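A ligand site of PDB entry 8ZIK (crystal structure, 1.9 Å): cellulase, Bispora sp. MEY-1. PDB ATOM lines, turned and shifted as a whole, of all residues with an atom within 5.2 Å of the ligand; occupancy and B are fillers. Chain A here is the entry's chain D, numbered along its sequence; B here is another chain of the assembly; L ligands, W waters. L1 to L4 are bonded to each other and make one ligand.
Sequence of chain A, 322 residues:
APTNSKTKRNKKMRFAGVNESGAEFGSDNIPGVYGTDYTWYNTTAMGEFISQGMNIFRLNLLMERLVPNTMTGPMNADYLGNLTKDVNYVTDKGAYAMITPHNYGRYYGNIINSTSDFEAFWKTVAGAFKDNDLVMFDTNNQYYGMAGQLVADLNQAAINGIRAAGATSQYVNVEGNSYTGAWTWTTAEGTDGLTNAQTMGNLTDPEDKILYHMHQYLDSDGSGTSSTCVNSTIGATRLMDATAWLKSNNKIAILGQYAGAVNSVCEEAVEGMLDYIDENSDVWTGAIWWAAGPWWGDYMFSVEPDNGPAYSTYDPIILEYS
OG of Ser 21 touches C5 of LIG L1 (3.9 Å).
Phe 25 touches the ligand.
O of Gly 35 touches C2 of LG4 L4, 3.8 Å away.
CZ2 of Trp 295 touches C4 of LG4 L4, 3.8 Å away.
CH2 of Trp 296 touches O5 of LIG L1, at 3.8 Å.
Within 4 Å of the ligand: Ser 21, Glu 24, Phe 25, Gly 26, Gly 35, Thr 36, Asp 37, His 102, Trp 290, Trp 295, Trp 296 and Tyr 299.
The nearest printed residue that does not touch the ligand is Tyr 104 (4.7 Å).
Water W2 lies within hydrogen-bond range of OD1 of Asp 37 (2.6 Å) and O5 of LG3 L3 (2.7 Å).
Water W3 lies within hydrogen-bond range of the side-chain hydroxyl of Tyr 104 (2.9 Å), an oxygen (O6) of LIG L1 (2.9 Å) and a ring nitrogen (NE2) of His 102 (3.3 Å).
Water W4 lies within hydrogen-bond range of NE2 of His 102 (2.8 Å), OH of Tyr 104 (3.0 Å) and O5 of LIG L1 (3.1 Å).
Water W6 lies within hydrogen-bond range of N of Ser 27 and O1 of LG2 L2.
The side-chain hydroxyl (OG) of Ser 21 is in hydrogen-bond range of the side-chain carboxylate (OE2) of Glu 24, 2.6 Å away.
The side-chain hydroxyl (OH) of Tyr 299 lies within hydrogen-bond range of the indole nitrogen (NE1) of Trp 290.
A ring nitrogen (NE2) of His 102 is in hydrogen-bond range of the side-chain hydroxyl (OH) of Tyr 104 (2.9 Å).
OE2 of Glu 24 is in hydrogen-bond range of O6 of LIG L1 (2.7 Å).
O of Asp 37 sits at hydrogen-bond distance from O5 of LG3 L3 (2.8 Å).
An oxygen (O1) of LG4 L4 sits at hydrogen-bond distance from the backbone carbonyl oxygen (O) of Thr 36, at 2.9 Å.
NE1 of Trp 290 lies within hydrogen-bond range of O1 of LIG L1.
N of Gly 26 lies within hydrogen-bond range of O2 of LG2 L2 (3.4 Å).
A ring nitrogen (NE2) of His 102 sits at hydrogen-bond distance from an oxygen (O6) of LIG L1.
The side-chain hydroxyl (OH) of Tyr 299 lies within hydrogen-bond range of an oxygen (O1) of LIG L1 (3.4 Å).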
ATOM      1  N   SER A  21     -28.092  -8.299 -17.291  1.00  0.00           N
ATOM      2  CA  SER A  21     -28.658  -8.042 -18.602  1.00  0.00           C
ATOM      3  C   SER A  21     -28.579  -9.320 -19.425  1.00  0.00           C
ATOM      4  O   SER A  21     -27.524  -9.968 -19.465  1.00  0.00           O
ATOM      5  CB  SER A  21     -27.909  -6.895 -19.288  1.00  0.00           C
ATOM      6  OG  SER A  21     -28.328  -6.688 -20.620  1.00  0.00           O
ATOM      7  N   GLU A  24     -33.668  -9.368 -21.495  1.00  0.00           N
ATOM      8  CA  GLU A  24     -34.239  -8.420 -22.422  1.00  0.00           C
ATOM      9  C   GLU A  24     -33.569  -8.473 -23.790  1.00  0.00           C
ATOM     10  O   GLU A  24     -33.888  -7.659 -24.672  1.00  0.00           O
ATOM     11  CB  GLU A  24     -34.153  -7.008 -21.828  1.00  0.00           C
ATOM     12  CG  GLU A  24     -32.848  -6.285 -22.094  1.00  0.00           C
ATOM     13  CD  GLU A  24     -31.732  -6.707 -21.144  1.00  0.00           C
ATOM     14  OE1 GLU A  24     -31.767  -7.839 -20.594  1.00  0.00           O
ATOM     15  OE2 GLU A  24     -30.804  -5.897 -20.940  1.00  0.00           O
ATOM     16  N   PHE A  25     -32.673  -9.440 -24.005  1.00  0.00           N
ATOM     17  CA  PHE A  25     -31.968  -9.579 -25.269  1.00  0.00           C
ATOM     18  C   PHE A  25     -32.914 -10.009 -26.389  1.00  0.00           C
ATOM     19  O   PHE A  25     -34.025 -10.502 -26.150  1.00  0.00           O
ATOM     20  CB  PHE A  25     -30.839 -10.601 -25.121  1.00  0.00           C
ATOM     21  CG  PHE A  25     -29.600 -10.058 -24.455  1.00  0.00           C
ATOM     22  CD1 PHE A  25     -29.633  -8.900 -23.693  1.00  0.00           C
ATOM     23  CD2 PHE A  25     -28.374 -10.714 -24.607  1.00  0.00           C
ATOM     24  CE1 PHE A  25     -28.482  -8.414 -23.085  1.00  0.00           C
ATOM     25  CE2 PHE A  25     -27.219 -10.226 -24.011  1.00  0.00           C
ATOM     26  CZ  PHE A  25     -27.274  -9.071 -23.250  1.00  0.00           C
ATOM     27  N   GLY A  26     -32.460  -9.820 -27.626  1.00  0.00           N
ATOM     28  CA  GLY A  26     -33.276 -10.220 -28.769  1.00  0.00           C
ATOM     29  C   GLY A  26     -34.648  -9.593 -28.733  1.00  0.00           C
ATOM     30  O   GLY A  26     -35.654 -10.266 -28.994  1.00  0.00           O
ATOM     31  N   SER A  27     -34.715  -8.307 -28.390  1.00  0.00           N
ATOM     32  CA  SER A  27     -35.981  -7.588 -28.317  1.00  0.00           C
ATOM     33  C   SER A  27     -36.764  -7.634 -29.625  1.00  0.00           C
ATOM     34  O   SER A  27     -37.964  -7.325 -29.631  1.00  0.00           O
ATOM     35  CB  SER A  27     -35.688  -6.153 -27.887  1.00  0.00           C
ATOM     36  OG  SER A  27     -36.594  -5.241 -28.481  1.00  0.00           O
ATOM     37  N   GLY A  35     -33.040 -19.346 -24.212  1.00  0.00           N
ATOM     38  CA  GLY A  35     -31.872 -20.060 -24.674  1.00  0.00           C
ATOM     39  C   GLY A  35     -31.449 -19.747 -26.082  1.00  0.00           C
ATOM     40  O   GLY A  35     -30.352 -20.162 -26.488  1.00  0.00           O
ATOM     41  N   THR A  36     -32.275 -19.049 -26.861  1.00  0.00           N
ATOM     42  CA  THR A  36     -31.854 -18.573 -28.173  1.00  0.00           C
ATOM     43  C   THR A  36     -31.879 -17.055 -28.286  1.00  0.00           C
ATOM     44  O   THR A  36     -30.889 -16.458 -28.719  1.00  0.00           O
ATOM     45  CB  THR A  36     -32.726 -19.165 -29.293  1.00  0.00           C
ATOM     46  OG1 THR A  36     -32.553 -20.587 -29.345  1.00  0.00           O
ATOM     47  CG2 THR A  36     -32.320 -18.576 -30.639  1.00  0.00           C
ATOM     48  N   ASP A  37     -32.996 -16.425 -27.932  1.00  0.00           N
ATOM     49  CA  ASP A  37     -33.106 -14.981 -28.036  1.00  0.00           C
ATOM     50  C   ASP A  37     -32.704 -14.273 -26.747  1.00  0.00           C
ATOM     51  O   ASP A  37     -32.087 -13.206 -26.790  1.00  0.00           O
ATOM     52  CB  ASP A  37     -34.529 -14.582 -28.420  1.00  0.00           C
ATOM     53  CG  ASP A  37     -34.963 -15.190 -29.735  1.00  0.00           C
ATOM     54  OD1 ASP A  37     -34.431 -14.755 -30.780  1.00  0.00           O
ATOM     55  OD2 ASP A  37     -35.802 -16.112 -29.718  1.00  0.00           O
ATOM     56  N   TYR A  38     -33.045 -14.855 -25.603  1.00  0.00           N
ATOM     57  CA  TYR A  38     -32.687 -14.253 -24.328  1.00  0.00           C
ATOM     58  C   TYR A  38     -32.303 -15.351 -23.353  1.00  0.00           C
ATOM     59  O   TYR A  38     -32.469 -16.542 -23.628  1.00  0.00           O
ATOM     60  CB  TYR A  38     -33.836 -13.403 -23.782  1.00  0.00           C
ATOM     61  CG  TYR A  38     -35.088 -14.226 -23.558  1.00  0.00           C
ATOM     62  CD1 TYR A  38     -35.966 -14.483 -24.596  1.00  0.00           C
ATOM     63  CD2 TYR A  38     -35.373 -14.740 -22.306  1.00  0.00           C
ATOM     64  CE1 TYR A  38     -37.123 -15.243 -24.385  1.00  0.00           C
ATOM     65  CE2 TYR A  38     -36.513 -15.488 -22.081  1.00  0.00           C
ATOM     66  CZ  TYR A  38     -37.384 -15.734 -23.123  1.00  0.00           C
ATOM     67  OH  TYR A  38     -38.519 -16.484 -22.867  1.00  0.00           O
ATOM     68  N   HIS A 102     -37.207  -3.345 -19.110  1.00  0.00           N
ATOM     69  CA  HIS A 102     -36.233  -2.612 -19.925  1.00  0.00           C
ATOM     70  C   HIS A 102     -36.898  -2.147 -21.223  1.00  0.00           C
ATOM     71  O   HIS A 102     -36.596  -2.608 -22.320  1.00  0.00           O
ATOM     72  CB  HIS A 102     -35.041  -3.503 -20.202  1.00  0.00           C
ATOM     73  CG  HIS A 102     -33.801  -2.774 -20.614  1.00  0.00           C
ATOM     74  ND1 HIS A 102     -32.817  -2.407 -19.730  1.00  0.00           N
ATOM     75  CD2 HIS A 102     -33.378  -2.377 -21.840  1.00  0.00           C
ATOM     76  CE1 HIS A 102     -31.837  -1.810 -20.383  1.00  0.00           C
ATOM     77  NE2 HIS A 102     -32.156  -1.777 -21.671  1.00  0.00           N
ATOM     78  N   TYR A 104     -37.982   1.427 -22.133  1.00  0.00           N
ATOM     79  CA  TYR A 104     -37.873   2.789 -22.659  1.00  0.00           C
ATOM     80  C   TYR A 104     -39.237   3.480 -22.738  1.00  0.00           C
ATOM     81  O   TYR A 104     -39.462   4.335 -23.601  1.00  0.00           O
ATOM     82  CB  TYR A 104     -37.187   2.781 -24.045  1.00  0.00           C
ATOM     83  CG  TYR A 104     -35.892   1.990 -24.068  1.00  0.00           C
ATOM     84  CD1 TYR A 104     -34.691   2.561 -23.641  1.00  0.00           C
ATOM     85  CD2 TYR A 104     -35.856   0.683 -24.542  1.00  0.00           C
ATOM     86  CE1 TYR A 104     -33.496   1.847 -23.654  1.00  0.00           C
ATOM     87  CE2 TYR A 104     -34.656  -0.039 -24.570  1.00  0.00           C
ATOM     88  CZ  TYR A 104     -33.486   0.536 -24.115  1.00  0.00           C
ATOM     89  OH  TYR A 104     -32.300  -0.180 -24.123  1.00  0.00           O
ATOM     90  N   TRP A 290     -23.076  -0.979 -15.175  1.00  0.00           N
ATOM     91  CA  TRP A 290     -23.604  -1.579 -16.384  1.00  0.00           C
ATOM     92  C   TRP A 290     -22.453  -2.164 -17.161  1.00  0.00           C
ATOM     93  O   TRP A 290     -21.637  -1.407 -17.701  1.00  0.00           O
ATOM     94  CB  TRP A 290     -24.377  -0.574 -17.238  1.00  0.00           C
ATOM     95  CG  TRP A 290     -24.888  -1.206 -18.513  1.00  0.00           C
ATOM     96  CD1 TRP A 290     -24.212  -1.356 -19.706  1.00  0.00           C
ATOM     97  CD2 TRP A 290     -26.178  -1.802 -18.702  1.00  0.00           C
ATOM     98  NE1 TRP A 290     -25.030  -2.001 -20.629  1.00  0.00           N
ATOM     99  CE2 TRP A 290     -26.231  -2.287 -20.032  1.00  0.00           C
ATOM    100  CE3 TRP A 290     -27.288  -1.977 -17.867  1.00  0.00           C
ATOM    101  CZ2 TRP A 290     -27.353  -2.921 -20.547  1.00  0.00           C
ATOM    102  CZ3 TRP A 290     -28.401  -2.609 -18.387  1.00  0.00           C
ATOM    103  CH2 TRP A 290     -28.426  -3.070 -19.720  1.00  0.00           C
ATOM    104  N   TRP A 295     -24.196 -13.525 -21.240  1.00  0.00           N
ATOM    105  CA  TRP A 295     -24.190 -13.574 -22.701  1.00  0.00           C
ATOM    106  C   TRP A 295     -23.531 -12.355 -23.315  1.00  0.00           C
ATOM    107  O   TRP A 295     -23.845 -12.011 -24.462  1.00  0.00           O
ATOM    108  CB  TRP A 295     -25.615 -13.687 -23.246  1.00  0.00           C
ATOM    109  CG  TRP A 295     -26.183 -15.065 -23.282  1.00  0.00           C
ATOM    110  CD1 TRP A 295     -25.720 -16.163 -22.619  1.00  0.00           C
ATOM    111  CD2 TRP A 295     -27.324 -15.496 -24.030  1.00  0.00           C
ATOM    112  NE1 TRP A 295     -26.513 -17.253 -22.902  1.00  0.00           N
ATOM    113  CE2 TRP A 295     -27.501 -16.872 -23.774  1.00  0.00           C
ATOM    114  CE3 TRP A 295     -28.221 -14.850 -24.897  1.00  0.00           C
ATOM    115  CZ2 TRP A 295     -28.537 -17.611 -24.337  1.00  0.00           C
ATOM    116  CZ3 TRP A 295     -29.247 -15.598 -25.466  1.00  0.00           C
ATOM    117  CH2 TRP A 295     -29.389 -16.961 -25.183  1.00  0.00           C
ATOM    118  N   TRP A 296     -22.646 -11.692 -22.585  1.00  0.00           N
ATOM    119  CA  TRP A 296     -22.045 -10.462 -23.066  1.00  0.00           C
ATOM    120  C   TRP A 296     -20.822 -10.704 -23.938  1.00  0.00           C
ATOM    121  O   TRP A 296     -20.459  -9.819 -24.735  1.00  0.00           O
ATOM    122  CB  TRP A 296     -21.668  -9.577 -21.872  1.00  0.00           C
ATOM    123  CG  TRP A 296     -22.766  -8.691 -21.306  1.00  0.00           C
ATOM    124  CD1 TRP A 296     -23.238  -8.676 -20.009  1.00  0.00           C
ATOM    125  CD2 TRP A 296     -23.495  -7.665 -22.002  1.00  0.00           C
ATOM    126  NE1 TRP A 296     -24.204  -7.703 -19.860  1.00  0.00           N
ATOM    127  CE2 TRP A 296     -24.388  -7.081 -21.078  1.00  0.00           C
ATOM    128  CE3 TRP A 296     -23.488  -7.201 -23.324  1.00  0.00           C
ATOM    129  CZ2 TRP A 296     -25.258  -6.047 -21.428  1.00  0.00           C
ATOM    130  CZ3 TRP A 296     -24.345  -6.165 -23.670  1.00  0.00           C
ATOM    131  CH2 TRP A 296     -25.235  -5.603 -22.725  1.00  0.00           C
ATOM    132  N   TYR A 299     -18.004  -7.807 -24.730  1.00  0.00           N
ATOM    133  CA  TYR A 299     -18.546  -6.482 -24.498  1.00  0.00           C
ATOM    134  C   TYR A 299     -17.609  -5.687 -23.600  1.00  0.00           C
ATOM    135  O   TYR A 299     -17.178  -6.177 -22.564  1.00  0.00           O
ATOM    136  CB  TYR A 299     -19.926  -6.613 -23.860  1.00  0.00           C
ATOM    137  CG  TYR A 299     -20.687  -5.331 -23.583  1.00  0.00           C
ATOM    138  CD1 TYR A 299     -20.831  -4.344 -24.551  1.00  0.00           C
ATOM    139  CD2 TYR A 299     -21.311  -5.126 -22.359  1.00  0.00           C
ATOM    140  CE1 TYR A 299     -21.552  -3.166 -24.298  1.00  0.00           C
ATOM    141  CE2 TYR A 299     -22.047  -3.971 -22.099  1.00  0.00           C
ATOM    142  CZ  TYR A 299     -22.166  -3.001 -23.069  1.00  0.00           C
ATOM    143  OH  TYR A 299     -22.888  -1.846 -22.783  1.00  0.00           O
ATOM    144  N   THR B 187     -29.085 -26.195 -28.375  1.00  0.00           N
ATOM    145  CA  THR B 187     -29.010 -25.562 -29.682  1.00  0.00           C
ATOM    146  C   THR B 187     -29.738 -26.310 -30.779  1.00  0.00           C
ATOM    147  O   THR B 187     -30.407 -25.679 -31.608  1.00  0.00           O
ATOM    148  CB  THR B 187     -27.535 -25.382 -30.076  1.00  0.00           C
ATOM    149  OG1 THR B 187     -26.915 -26.672 -30.144  1.00  0.00           O
ATOM    150  CG2 THR B 187     -26.825 -24.528 -29.045  1.00  0.00           C
HETATM  151  C1  LIG L   1     -26.019  -2.559 -25.490  1.00  0.00           C
HETATM  152  C2  LIG L   1     -26.766  -3.441 -26.491  1.00  0.00           C
HETATM  153  C3  LIG L   1     -27.606  -4.475 -25.743  1.00  0.00           C
HETATM  154  C4  LIG L   1     -28.494  -3.748 -24.715  1.00  0.00           C
HETATM  155  C5  LIG L   1     -29.219  -4.788 -23.858  1.00  0.00           C
HETATM  156  C6  LIG L   1     -26.970  -1.911 -24.477  1.00  0.00           C
HETATM  157  O1  LIG L   1     -26.174  -1.239 -23.542  1.00  0.00           O
HETATM  158  O2  LIG L   1     -25.271  -1.575 -26.168  1.00  0.00           O
HETATM  159  O3  LIG L   1     -25.827  -4.023 -27.371  1.00  0.00           O
HETATM  160  O4  LIG L   1     -28.335  -5.141 -26.746  1.00  0.00           O
HETATM  161  O5  LIG L   1     -27.727  -2.930 -23.873  1.00  0.00           O
HETATM  162  O6  LIG L   1     -30.095  -4.169 -22.954  1.00  0.00           O
HETATM  163  C1  LG2 L   2     -28.862  -7.402 -27.541  1.00  0.00           C
HETATM  164  C2  LG2 L   2     -28.420  -8.873 -27.555  1.00  0.00           C
HETATM  165  C3  LG2 L   2     -26.933  -8.964 -27.952  1.00  0.00           C
HETATM  166  C4  LG2 L   2     -26.150  -8.019 -27.035  1.00  0.00           C
HETATM  167  C5  LG2 L   2     -24.616  -8.041 -27.251  1.00  0.00           C
HETATM  168  C6  LG2 L   2     -27.971  -6.499 -26.671  1.00  0.00           C
HETATM  169  O1  LG2 L   2     -30.184  -7.334 -27.096  1.00  0.00           O
HETATM  170  O2  LG2 L   2     -29.210  -9.521 -28.515  1.00  0.00           O
HETATM  171  O3  LG2 L   2     -26.423 -10.247 -27.725  1.00  0.00           O
HETATM  172  O4  LG2 L   2     -26.659  -6.698 -27.137  1.00  0.00           O
HETATM  173  O5  LG2 L   2     -24.287  -7.445 -28.456  1.00  0.00           O
HETATM  174  C1  LG3 L   3     -25.410 -12.033 -28.837  1.00  0.00           C
HETATM  175  C2  LG3 L   3     -25.652 -13.424 -29.439  1.00  0.00           C
HETATM  176  C3  LG3 L   3     -26.944 -14.057 -28.940  1.00  0.00           C
HETATM  177  C4  LG3 L   3     -28.060 -13.072 -29.208  1.00  0.00           C
HETATM  178  C5  LG3 L   3     -29.417 -13.588 -28.750  1.00  0.00           C
HETATM  179  C6  LG3 L   3     -26.658 -11.148 -28.779  1.00  0.00           C
HETATM  180  O1  LG3 L   3     -24.411 -11.381 -29.611  1.00  0.00           O
HETATM  181  O2  LG3 L   3     -24.511 -14.189 -29.110  1.00  0.00           O
HETATM  182  O3  LG3 L   3     -27.133 -15.213 -29.709  1.00  0.00           O
HETATM  183  O4  LG3 L   3     -27.806 -11.894 -28.483  1.00  0.00           O
HETATM  184  O5  LG3 L   3     -30.374 -12.566 -28.875  1.00  0.00           O
HETATM  185  C1  LG4 L   4     -27.589 -17.542 -29.708  1.00  0.00           C
HETATM  186  C2  LG4 L   4     -27.728 -18.746 -28.767  1.00  0.00           C
HETATM  187  C3  LG4 L   4     -26.421 -18.953 -28.011  1.00  0.00           C
HETATM  188  C4  LG4 L   4     -26.077 -17.674 -27.251  1.00  0.00           C
HETATM  189  C5  LG4 L   4     -24.699 -17.811 -26.598  1.00  0.00           C
HETATM  190  C6  LG4 L   4     -27.270 -16.306 -28.857  1.00  0.00           C
HETATM  191  O1  LG4 L   4     -28.751 -17.375 -30.484  1.00  0.00           O
HETATM  192  O2  LG4 L   4     -28.077 -19.884 -29.509  1.00  0.00           O
HETATM  193  O3  LG4 L   4     -26.546 -20.029 -27.108  1.00  0.00           O
HETATM  194  O4  LG4 L   4     -26.079 -16.557 -28.121  1.00  0.00           O
HETATM  195  O5  LG4 L   4     -24.142 -16.544 -26.379  1.00  0.00           O
HETATM  196  O   HOH W   1     -27.354   1.242 -21.781  1.00  0.00           O
HETATM  197  O   HOH W   2     -32.211 -13.451 -30.684  1.00  0.00           O
HETATM  198  O   HOH W   3     -32.078  -2.984 -24.784  1.00  0.00           O
HETATM  199  O   HOH W   4     -29.703  -0.857 -22.735  1.00  0.00           O
HETATM  200  O   HOH W   5     -30.495  -7.983 -30.745  1.00  0.00           O
HETATM  201  O   HOH W   6     -32.590  -6.530 -28.908  1.00  0.00           O
